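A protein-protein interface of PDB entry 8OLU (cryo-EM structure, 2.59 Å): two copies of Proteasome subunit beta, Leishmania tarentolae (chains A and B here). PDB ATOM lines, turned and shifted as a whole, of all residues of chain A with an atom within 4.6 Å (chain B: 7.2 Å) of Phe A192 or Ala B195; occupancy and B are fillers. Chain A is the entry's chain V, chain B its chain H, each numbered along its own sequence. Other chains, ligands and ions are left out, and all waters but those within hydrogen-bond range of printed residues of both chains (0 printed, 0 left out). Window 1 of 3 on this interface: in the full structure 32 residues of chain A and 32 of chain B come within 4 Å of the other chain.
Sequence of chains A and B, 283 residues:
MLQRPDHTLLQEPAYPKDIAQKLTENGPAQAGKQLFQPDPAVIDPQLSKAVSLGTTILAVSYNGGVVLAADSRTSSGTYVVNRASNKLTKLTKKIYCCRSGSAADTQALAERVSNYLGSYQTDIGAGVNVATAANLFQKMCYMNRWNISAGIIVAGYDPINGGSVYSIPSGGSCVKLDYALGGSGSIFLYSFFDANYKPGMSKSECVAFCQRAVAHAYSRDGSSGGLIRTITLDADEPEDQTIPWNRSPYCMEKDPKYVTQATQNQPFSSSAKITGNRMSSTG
Ser A191 touches His B216. Phe A192 touches Ala B195. ND1 of His B216 touches CB of Asp A194 (3.7 Å). CE1 of Phe B192 touches CB of Ala A195 (3.6 Å). N of Ala A195 touches CE1 of His B216, at 3.7 Å. OG of Ser B191 touches O of His A216, at 3.8 Å. ND1 of His A216 touches CB of Asp B194, 3.7 Å away. CE1 of His A216 touches N of Ala B195, at 3.7 Å.
Of the 14 printed residues of chain A, 9 touch a printed residue of chain B. Printed residues of chain A that touch a printed residue of chain B: Phe A188, Ser A191, Phe A192, Phe A193, Asp A194, Ala A195, Asn A196, Tyr A197 and His A216. Hydrophobic or aromatic side chains of chain A within 4 Å of the printed part of chain B: Phe A188, Phe A192, Ala A195, Tyr A197 and His A216. Among the printed residues, no Asp or Glu carboxylate lies within 4 Å of a Lys or Arg side-chain nitrogen of the other chain.
Of chain B, only Ala B195 comes within 4 Å of Phe A192. Ala B195 touches just these residues of chain A: Phe A192 and His A216. Of the printed residues of chain A, Asn B196 touches Asn A196 (3.0 Å). Of the printed residues of chain B, Ala A195 touches Phe B192 (3.6 Å) and His B216 (3.7 Å). Of the printed residues of chain B, His A216 touches Ser B191, Asp B194 and Ala B195. Of the printed residues of chain A, Asp B194 touches His A216. The nearest residue of chain A that does not touch Ala B195 is Asn A196 (4.2 Å).
O of Phe B192 lies close to OD1 of Asn B196, 3.3 Å away. The side-chain amide oxygen (OD1) of Asn A196 lies close to the backbone carbonyl oxygen (O) of Phe A192 (3.3 Å).
OG of Ser A191 lies close to O of Phe B188 (3.1 Å). OG of Ser B191 lies close to O of Phe A188, 3.1 Å away. The side-chain amide nitrogen of Asn B196 lies close to the side-chain amide nitrogen of Asn A196 (3.0 Å). The backbone carbonyl oxygen of Phe A193 sits at hydrogen-bond distance from the side-chain amino group of Lys B257, 3.2 Å away. NZ of Lys B257 sits at hydrogen-bond distance from O of Asp A194, 2.9 Å away. NZ of Lys B257 lies within hydrogen-bond range of O of Tyr A197.
Phe A188 touches Ser B191, and with the chains exchanged Ser A191 touches Phe B188. Phe A192 touches Ala B195, and with the chains exchanged Ala A195 touches Phe B192. Ala A195 touches His B216, and with the chains exchanged His A216 touches Ala B195. Asn B196 touches its own counterpart, Asn A196.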
ATOM      1  N   PHE A 188      18.804  14.972  -1.220  1.00  0.00           N
ATOM      2  CA  PHE A 188      19.136  13.925  -0.276  1.00  0.00           C
ATOM      3  C   PHE A 188      18.517  14.089   1.089  1.00  0.00           C
ATOM      4  O   PHE A 188      18.554  13.168   1.865  1.00  0.00           O
ATOM      5  CB  PHE A 188      20.633  13.913   0.007  1.00  0.00           C
ATOM      6  CG  PHE A 188      21.366  13.589  -1.259  1.00  0.00           C
ATOM      7  CD1 PHE A 188      21.237  12.358  -1.823  1.00  0.00           C
ATOM      8  CD2 PHE A 188      22.048  14.540  -1.959  1.00  0.00           C
ATOM      9  CE1 PHE A 188      21.854  12.062  -3.031  1.00  0.00           C
ATOM     10  CE2 PHE A 188      22.602  14.273  -3.195  1.00  0.00           C
ATOM     11  CZ  PHE A 188      22.542  13.022  -3.721  1.00  0.00           C
ATOM     12  N   LEU A 189      17.938  15.205   1.424  1.00  0.00           N
ATOM     13  CA  LEU A 189      17.471  15.384   2.777  1.00  0.00           C
ATOM     14  C   LEU A 189      15.972  15.271   2.897  1.00  0.00           C
ATOM     15  O   LEU A 189      15.427  15.215   3.971  1.00  0.00           O
ATOM     16  CB  LEU A 189      17.875  16.800   3.133  1.00  0.00           C
ATOM     17  CG  LEU A 189      19.363  16.979   3.330  1.00  0.00           C
ATOM     18  CD1 LEU A 189      19.668  18.223   4.115  1.00  0.00           C
ATOM     19  CD2 LEU A 189      19.850  15.761   4.068  1.00  0.00           C
ATOM     20  N   TYR A 190      15.258  15.331   1.810  1.00  0.00           N
ATOM     21  CA  TYR A 190      13.831  15.223   1.898  1.00  0.00           C
ATOM     22  C   TYR A 190      13.408  14.000   2.668  1.00  0.00           C
ATOM     23  O   TYR A 190      12.735  14.092   3.649  1.00  0.00           O
ATOM     24  CB  TYR A 190      13.287  15.241   0.489  1.00  0.00           C
ATOM     25  CG  TYR A 190      13.242  16.635  -0.031  1.00  0.00           C
ATOM     26  CD1 TYR A 190      12.476  17.570   0.630  1.00  0.00           C
ATOM     27  CD2 TYR A 190      13.999  17.031  -1.117  1.00  0.00           C
ATOM     28  CE1 TYR A 190      12.405  18.882   0.187  1.00  0.00           C
ATOM     29  CE2 TYR A 190      13.952  18.357  -1.553  1.00  0.00           C
ATOM     30  CZ  TYR A 190      13.161  19.290  -0.886  1.00  0.00           C
ATOM     31  OH  TYR A 190      13.101  20.637  -1.281  1.00  0.00           O
ATOM     32  N   SER A 191      13.831  12.836   2.268  1.00  0.00           N
ATOM     33  CA  SER A 191      13.545  11.642   3.050  1.00  0.00           C
ATOM     34  C   SER A 191      14.125  11.711   4.440  1.00  0.00           C
ATOM     35  O   SER A 191      13.508  11.235   5.365  1.00  0.00           O
ATOM     36  CB  SER A 191      14.040  10.449   2.348  1.00  0.00           C
ATOM     37  OG  SER A 191      13.132  10.197   1.245  1.00  0.00           O
ATOM     38  N   PHE A 192      15.285  12.296   4.608  1.00  0.00           N
ATOM     39  CA  PHE A 192      15.832  12.390   5.938  1.00  0.00           C
ATOM     40  C   PHE A 192      14.924  13.180   6.880  1.00  0.00           C
ATOM     41  O   PHE A 192      14.676  12.825   8.001  1.00  0.00           O
ATOM     42  CB  PHE A 192      17.161  13.102   5.780  1.00  0.00           C
ATOM     43  CG  PHE A 192      17.930  13.170   7.044  1.00  0.00           C
ATOM     44  CD1 PHE A 192      18.507  12.033   7.545  1.00  0.00           C
ATOM     45  CD2 PHE A 192      17.977  14.345   7.758  1.00  0.00           C
ATOM     46  CE1 PHE A 192      19.171  12.078   8.751  1.00  0.00           C
ATOM     47  CE2 PHE A 192      18.626  14.375   8.987  1.00  0.00           C
ATOM     48  CZ  PHE A 192      19.228  13.244   9.469  1.00  0.00           C
ATOM     49  N   PHE A 193      14.360  14.263   6.403  1.00  0.00           N
ATOM     50  CA  PHE A 193      13.423  15.011   7.190  1.00  0.00           C
ATOM     51  C   PHE A 193      12.102  14.284   7.369  1.00  0.00           C
ATOM     52  O   PHE A 193      11.545  14.241   8.467  1.00  0.00           O
ATOM     53  CB  PHE A 193      13.216  16.336   6.494  1.00  0.00           C
ATOM     54  CG  PHE A 193      14.237  17.329   6.938  1.00  0.00           C
ATOM     55  CD1 PHE A 193      15.513  17.280   6.450  1.00  0.00           C
ATOM     56  CD2 PHE A 193      13.897  18.322   7.851  1.00  0.00           C
ATOM     57  CE1 PHE A 193      16.459  18.164   6.907  1.00  0.00           C
ATOM     58  CE2 PHE A 193      14.862  19.194   8.333  1.00  0.00           C
ATOM     59  CZ  PHE A 193      16.146  19.087   7.866  1.00  0.00           C
ATOM     60  N   ASP A 194      11.538  13.830   6.268  1.00  0.00           N
ATOM     61  CA  ASP A 194      10.346  13.020   6.327  1.00  0.00           C
ATOM     62  C   ASP A 194      10.519  11.942   7.383  1.00  0.00           C
ATOM     63  O   ASP A 194       9.676  11.724   8.233  1.00  0.00           O
ATOM     64  CB  ASP A 194      10.071  12.418   4.964  1.00  0.00           C
ATOM     65  CG  ASP A 194       9.561  13.380   3.886  1.00  0.00           C
ATOM     66  OD1 ASP A 194       9.498  14.625   4.136  1.00  0.00           O
ATOM     67  OD2 ASP A 194       9.299  12.894   2.736  1.00  0.00           O
ATOM     68  N   ALA A 195      11.679  11.302   7.416  1.00  0.00           N
ATOM     69  CA  ALA A 195      11.813  10.189   8.333  1.00  0.00           C
ATOM     70  C   ALA A 195      12.242  10.577   9.739  1.00  0.00           C
ATOM     71  O   ALA A 195      11.816   9.927  10.658  1.00  0.00           O
ATOM     72  CB  ALA A 195      12.756   9.182   7.761  1.00  0.00           C
ATOM     73  N   ASN A 196      13.120  11.553   9.898  1.00  0.00           N
ATOM     74  CA  ASN A 196      13.817  11.745  11.157  1.00  0.00           C
ATOM     75  C   ASN A 196      13.562  13.107  11.811  1.00  0.00           C
ATOM     76  O   ASN A 196      13.872  13.282  12.982  1.00  0.00           O
ATOM     77  CB  ASN A 196      15.340  11.667  10.988  1.00  0.00           C
ATOM     78  CG  ASN A 196      15.773  10.373  10.377  1.00  0.00           C
ATOM     79  OD1 ASN A 196      16.378  10.355   9.316  1.00  0.00           O
ATOM     80  ND2 ASN A 196      15.402   9.286  11.014  1.00  0.00           N
ATOM     81  N   TYR A 197      13.004  14.067  11.094  1.00  0.00           N
ATOM     82  CA  TYR A 197      12.723  15.355  11.694  1.00  0.00           C
ATOM     83  C   TYR A 197      11.395  15.395  12.395  1.00  0.00           C
ATOM     84  O   TYR A 197      10.376  15.330  11.753  1.00  0.00           O
ATOM     85  CB  TYR A 197      12.632  16.405  10.595  1.00  0.00           C
ATOM     86  CG  TYR A 197      12.218  17.769  11.054  1.00  0.00           C
ATOM     87  CD1 TYR A 197      13.061  18.567  11.797  1.00  0.00           C
ATOM     88  CD2 TYR A 197      10.984  18.278  10.679  1.00  0.00           C
ATOM     89  CE1 TYR A 197      12.656  19.822  12.218  1.00  0.00           C
ATOM     90  CE2 TYR A 197      10.589  19.564  11.017  1.00  0.00           C
ATOM     91  CZ  TYR A 197      11.438  20.339  11.800  1.00  0.00           C
ATOM     92  OH  TYR A 197      10.981  21.599  12.151  1.00  0.00           O
ATOM     93  N   PHE A 209      20.561  18.535  14.844  1.00  0.00           N
ATOM     94  CA  PHE A 209      19.862  17.923  13.759  1.00  0.00           C
ATOM     95  C   PHE A 209      20.215  18.550  12.412  1.00  0.00           C
ATOM     96  O   PHE A 209      20.417  17.863  11.430  1.00  0.00           O
ATOM     97  CB  PHE A 209      18.391  18.133  13.980  1.00  0.00           C
ATOM     98  CG  PHE A 209      17.630  17.427  12.923  1.00  0.00           C
ATOM     99  CD1 PHE A 209      17.384  16.077  13.044  1.00  0.00           C
ATOM    100  CD2 PHE A 209      17.262  18.071  11.761  1.00  0.00           C
ATOM    101  CE1 PHE A 209      16.654  15.407  12.067  1.00  0.00           C
ATOM    102  CE2 PHE A 209      16.551  17.405  10.775  1.00  0.00           C
ATOM    103  CZ  PHE A 209      16.271  16.069  10.930  1.00  0.00           C
ATOM    104  N   ARG A 212      23.463  17.287  11.456  1.00  0.00           N
ATOM    105  CA  ARG A 212      23.454  15.930  10.967  1.00  0.00           C
ATOM    106  C   ARG A 212      22.942  15.956   9.531  1.00  0.00           C
ATOM    107  O   ARG A 212      23.412  15.263   8.655  1.00  0.00           O
ATOM    108  CB  ARG A 212      22.518  15.090  11.814  1.00  0.00           C
ATOM    109  CG  ARG A 212      23.168  13.816  12.302  1.00  0.00           C
ATOM    110  CD  ARG A 212      22.238  13.086  13.238  1.00  0.00           C
ATOM    111  NE  ARG A 212      21.389  12.164  12.475  1.00  0.00           N
ATOM    112  CZ  ARG A 212      20.117  11.843  12.756  1.00  0.00           C
ATOM    113  NH1 ARG A 212      19.330  12.649  13.487  1.00  0.00           N
ATOM    114  NH2 ARG A 212      19.649  10.720  12.229  1.00  0.00           N
ATOM    115  N   ALA A 213      21.908  16.743   9.323  1.00  0.00           N
ATOM    116  CA  ALA A 213      21.265  16.780   8.058  1.00  0.00           C
ATOM    117  C   ALA A 213      22.244  17.279   7.038  1.00  0.00           C
ATOM    118  O   ALA A 213      22.444  16.645   6.022  1.00  0.00           O
ATOM    119  CB  ALA A 213      20.076  17.658   8.093  1.00  0.00           C
ATOM    120  N   HIS A 216      24.766  14.407   6.242  1.00  0.00           N
ATOM    121  CA  HIS A 216      24.179  13.403   5.401  1.00  0.00           C
ATOM    122  C   HIS A 216      24.117  13.875   3.980  1.00  0.00           C
ATOM    123  O   HIS A 216      24.524  13.192   3.084  1.00  0.00           O
ATOM    124  CB  HIS A 216      22.797  13.056   5.920  1.00  0.00           C
ATOM    125  CG  HIS A 216      22.909  11.948   6.910  1.00  0.00           C
ATOM    126  ND1 HIS A 216      23.366  10.711   6.559  1.00  0.00           N
ATOM    127  CD2 HIS A 216      22.852  12.003   8.254  1.00  0.00           C
ATOM    128  CE1 HIS A 216      23.456   9.970   7.658  1.00  0.00           C
ATOM    129  NE2 HIS A 216      23.128  10.753   8.732  1.00  0.00           N
ATOM    130  N   PHE B 188      16.438   9.651  -3.270  1.00  0.00           N
ATOM    131  CA  PHE B 188      15.845   9.955  -1.985  1.00  0.00           C
ATOM    132  C   PHE B 188      16.178   8.972  -0.889  1.00  0.00           C
ATOM    133  O   PHE B 188      15.916   9.256   0.251  1.00  0.00           O
ATOM    134  CB  PHE B 188      14.325   9.902  -2.068  1.00  0.00           C
ATOM    135  CG  PHE B 188      13.852  10.963  -3.014  1.00  0.00           C
ATOM    136  CD1 PHE B 188      14.009  12.277  -2.696  1.00  0.00           C
ATOM    137  CD2 PHE B 188      13.396  10.663  -4.263  1.00  0.00           C
ATOM    138  CE1 PHE B 188      13.638  13.274  -3.589  1.00  0.00           C
ATOM    139  CE2 PHE B 188      13.094  11.648  -5.183  1.00  0.00           C
ATOM    140  CZ  PHE B 188      13.177  12.959  -4.837  1.00  0.00           C
ATOM    141  N   LEU B 189      16.749   7.839  -1.169  1.00  0.00           N
ATOM    142  CA  LEU B 189      16.936   6.861  -0.125  1.00  0.00           C
ATOM    143  C   LEU B 189      18.366   6.776   0.347  1.00  0.00           C
ATOM    144  O   LEU B 189      18.670   6.149   1.330  1.00  0.00           O
ATOM    145  CB  LEU B 189      16.566   5.542  -0.770  1.00  0.00           C
ATOM    146  CG  LEU B 189      15.086   5.385  -1.035  1.00  0.00           C
ATOM    147  CD1 LEU B 189      14.711   3.943  -1.225  1.00  0.00           C
ATOM    148  CD2 LEU B 189      14.371   5.958   0.160  1.00  0.00           C
ATOM    149  N   TYR B 190      19.294   7.323  -0.386  1.00  0.00           N
ATOM    150  CA  TYR B 190      20.661   7.259   0.042  1.00  0.00           C
ATOM    151  C   TYR B 190      20.828   7.754   1.454  1.00  0.00           C
ATOM    152  O   TYR B 190      21.284   7.052   2.304  1.00  0.00           O
ATOM    153  CB  TYR B 190      21.486   8.040  -0.954  1.00  0.00           C
ATOM    154  CG  TYR B 190      21.734   7.223  -2.174  1.00  0.00           C
ATOM    155  CD1 TYR B 190      22.410   6.029  -2.054  1.00  0.00           C
ATOM    156  CD2 TYR B 190      21.248   7.601  -3.411  1.00  0.00           C
ATOM    157  CE1 TYR B 190      22.663   5.233  -3.160  1.00  0.00           C
ATOM    158  CE2 TYR B 190      21.478   6.792  -4.527  1.00  0.00           C
ATOM    159  CZ  TYR B 190      22.175   5.593  -4.396  1.00  0.00           C
ATOM    160  OH  TYR B 190      22.407   4.738  -5.488  1.00  0.00           O
ATOM    161  N   SER B 191      20.418   8.955   1.745  1.00  0.00           N
ATOM    162  CA  SER B 191      20.450   9.429   3.121  1.00  0.00           C
ATOM    163  C   SER B 191      19.599   8.592   4.041  1.00  0.00           C
ATOM    164  O   SER B 191      19.975   8.385   5.171  1.00  0.00           O
ATOM    165  CB  SER B 191      20.031  10.838   3.178  1.00  0.00           C
ATOM    166  OG  SER B 191      21.128  11.630   2.659  1.00  0.00           O
ATOM    167  N   PHE B 192      18.473   8.103   3.585  1.00  0.00           N
ATOM    168  CA  PHE B 192      17.670   7.277   4.450  1.00  0.00           C
ATOM    169  C   PHE B 192      18.415   6.021   4.903  1.00  0.00           C
ATOM    170  O   PHE B 192      18.400   5.626   6.037  1.00  0.00           O
ATOM    171  CB  PHE B 192      16.455   6.892   3.628  1.00  0.00           C
ATOM    172  CG  PHE B 192      15.447   6.141   4.410  1.00  0.00           C
ATOM    173  CD1 PHE B 192      14.700   6.797   5.356  1.00  0.00           C
ATOM    174  CD2 PHE B 192      15.333   4.779   4.260  1.00  0.00           C
ATOM    175  CE1 PHE B 192      13.805   6.091   6.128  1.00  0.00           C
ATOM    176  CE2 PHE B 192      14.447   4.070   5.063  1.00  0.00           C
ATOM    177  CZ  PHE B 192      13.681   4.735   5.983  1.00  0.00           C
ATOM    178  N   PHE B 193      19.138   5.395   4.008  1.00  0.00           N
ATOM    179  CA  PHE B 193      19.941   4.264   4.373  1.00  0.00           C
ATOM    180  C   PHE B 193      21.142   4.650   5.219  1.00  0.00           C
ATOM    181  O   PHE B 193      21.454   3.996   6.215  1.00  0.00           O
ATOM    182  CB  PHE B 193      20.381   3.599   3.089  1.00  0.00           C
ATOM    183  CG  PHE B 193      19.360   2.609   2.633  1.00  0.00           C
ATOM    184  CD1 PHE B 193      18.213   3.027   2.017  1.00  0.00           C
ATOM    185  CD2 PHE B 193      19.569   1.248   2.828  1.00  0.00           C
ATOM    186  CE1 PHE B 193      17.256   2.111   1.652  1.00  0.00           C
ATOM    187  CE2 PHE B 193      18.589   0.331   2.484  1.00  0.00           C
ATOM    188  CZ  PHE B 193      17.426   0.781   1.917  1.00  0.00           C
ATOM    189  N   ASP B 194      21.890   5.629   4.748  1.00  0.00           N
ATOM    190  CA  ASP B 194      22.985   6.161   5.523  1.00  0.00           C
ATOM    191  C   ASP B 194      22.520   6.412   6.948  1.00  0.00           C
ATOM    192  O   ASP B 194      23.145   6.017   7.917  1.00  0.00           O
ATOM    193  CB  ASP B 194      23.495   7.432   4.874  1.00  0.00           C
ATOM    194  CG  ASP B 194      24.283   7.264   3.573  1.00  0.00           C
ATOM    195  OD1 ASP B 194      24.379   6.113   3.040  1.00  0.00           O
ATOM    196  OD2 ASP B 194      24.743   8.319   3.021  1.00  0.00           O
ATOM    197  N   ALA B 195      21.339   6.990   7.109  1.00  0.00           N
ATOM    198  CA  ALA B 195      20.938   7.349   8.452  1.00  0.00           C
ATOM    199  C   ALA B 195      20.255   6.233   9.229  1.00  0.00           C
ATOM    200  O   ALA B 195      20.435   6.183  10.418  1.00  0.00           O
ATOM    201  CB  ALA B 195      20.066   8.562   8.410  1.00  0.00           C
ATOM    202  N   ASN B 196      19.432   5.416   8.593  1.00  0.00           N
ATOM    203  CA  ASN B 196      18.504   4.563   9.314  1.00  0.00           C
ATOM    204  C   ASN B 196      18.709   3.064   9.070  1.00  0.00           C
ATOM    205  O   ASN B 196      18.177   2.250   9.815  1.00  0.00           O
ATOM    206  CB  ASN B 196      17.048   4.833   8.909  1.00  0.00           C
ATOM    207  CG  ASN B 196      16.660   6.262   9.111  1.00  0.00           C
ATOM    208  OD1 ASN B 196      16.297   6.950   8.170  1.00  0.00           O
ATOM    209  ND2 ASN B 196      16.806   6.728  10.331  1.00  0.00           N
ATOM    210  N   TYR B 197      19.472   2.680   8.060  1.00  0.00           N
ATOM    211  CA  TYR B 197      19.711   1.271   7.823  1.00  0.00           C
ATOM    212  C   TYR B 197      20.864   0.731   8.620  1.00  0.00           C
ATOM    213  O   TYR B 197      21.988   1.089   8.367  1.00  0.00           O
ATOM    214  CB  TYR B 197      20.097   1.074   6.364  1.00  0.00           C
ATOM    215  CG  TYR B 197      20.501  -0.322   5.997  1.00  0.00           C
ATOM    216  CD1 TYR B 197      19.579  -1.343   5.928  1.00  0.00           C
ATOM    217  CD2 TYR B 197      21.818  -0.591   5.660  1.00  0.00           C
ATOM    218  CE1 TYR B 197      19.976  -2.628   5.594  1.00  0.00           C
ATOM    219  CE2 TYR B 197      22.223  -1.849   5.245  1.00  0.00           C
ATOM    220  CZ  TYR B 197      21.287  -2.876   5.216  1.00  0.00           C
ATOM    221  OH  TYR B 197      21.752  -4.121   4.831  1.00  0.00           O
ATOM    222  N   LYS B 198      20.601  -0.135   9.564  1.00  0.00           N
ATOM    223  CA  LYS B 198      21.680  -0.916  10.133  1.00  0.00           C
ATOM    224  C   LYS B 198      21.589  -2.276   9.506  1.00  0.00           C
ATOM    225  O   LYS B 198      20.507  -2.856   9.512  1.00  0.00           O
ATOM    226  CB  LYS B 198      21.604  -1.037  11.656  1.00  0.00           C
ATOM    227  CG  LYS B 198      22.792  -0.423  12.407  1.00  0.00           C
ATOM    228  CD  LYS B 198      22.359   0.592  13.453  1.00  0.00           C
ATOM    229  CE  LYS B 198      21.569   1.740  12.840  1.00  0.00           C
ATOM    230  NZ  LYS B 198      20.245   1.895  13.490  1.00  0.00           N
ATOM    231  N   PHE B 209      11.628  -2.599   6.759  1.00  0.00           N
ATOM    232  CA  PHE B 209      12.496  -1.517   6.418  1.00  0.00           C
ATOM    233  C   PHE B 209      12.474  -1.198   4.925  1.00  0.00           C
ATOM    234  O   PHE B 209      12.432  -0.052   4.524  1.00  0.00           O
ATOM    235  CB  PHE B 209      13.900  -1.919   6.771  1.00  0.00           C
ATOM    236  CG  PHE B 209      14.811  -0.780   6.526  1.00  0.00           C
ATOM    237  CD1 PHE B 209      14.933   0.215   7.472  1.00  0.00           C
ATOM    238  CD2 PHE B 209      15.456  -0.631   5.316  1.00  0.00           C
ATOM    239  CE1 PHE B 209      15.801   1.281   7.260  1.00  0.00           C
ATOM    240  CE2 PHE B 209      16.310   0.438   5.094  1.00  0.00           C
ATOM    241  CZ  PHE B 209      16.457   1.399   6.063  1.00  0.00           C
ATOM    242  N   HIS B 216       9.029   6.098   1.632  1.00  0.00           N
ATOM    243  CA  HIS B 216       9.708   7.361   1.694  1.00  0.00           C
ATOM    244  C   HIS B 216      10.096   7.822   0.322  1.00  0.00           C
ATOM    245  O   HIS B 216       9.833   8.927  -0.057  1.00  0.00           O
ATOM    246  CB  HIS B 216      10.924   7.236   2.592  1.00  0.00           C
ATOM    247  CG  HIS B 216      10.531   7.548   3.996  1.00  0.00           C
ATOM    248  ND1 HIS B 216      10.074   8.780   4.360  1.00  0.00           N
ATOM    249  CD2 HIS B 216      10.309   6.703   5.020  1.00  0.00           C
ATOM    250  CE1 HIS B 216       9.704   8.730   5.635  1.00  0.00           C
ATOM    251  NE2 HIS B 216       9.855   7.442   6.077  1.00  0.00           N
ATOM    252  N   LYS B 257       3.539  16.190  10.712  1.00  0.00           N
ATOM    253  CA  LYS B 257       4.254  17.433  10.522  1.00  0.00           C
ATOM    254  C   LYS B 257       3.976  18.118   9.197  1.00  0.00           C
ATOM    255  O   LYS B 257       4.632  19.100   8.913  1.00  0.00           O
ATOM    256  CB  LYS B 257       5.753  17.214  10.641  1.00  0.00           C
ATOM    257  CG  LYS B 257       6.408  16.518   9.470  1.00  0.00           C
ATOM    258  CD  LYS B 257       7.921  16.493   9.560  1.00  0.00           C
ATOM    259  CE  LYS B 257       8.519  15.408   8.680  1.00  0.00           C
ATOM    260  NZ  LYS B 257       8.496  14.099   9.367  1.00  0.00           N
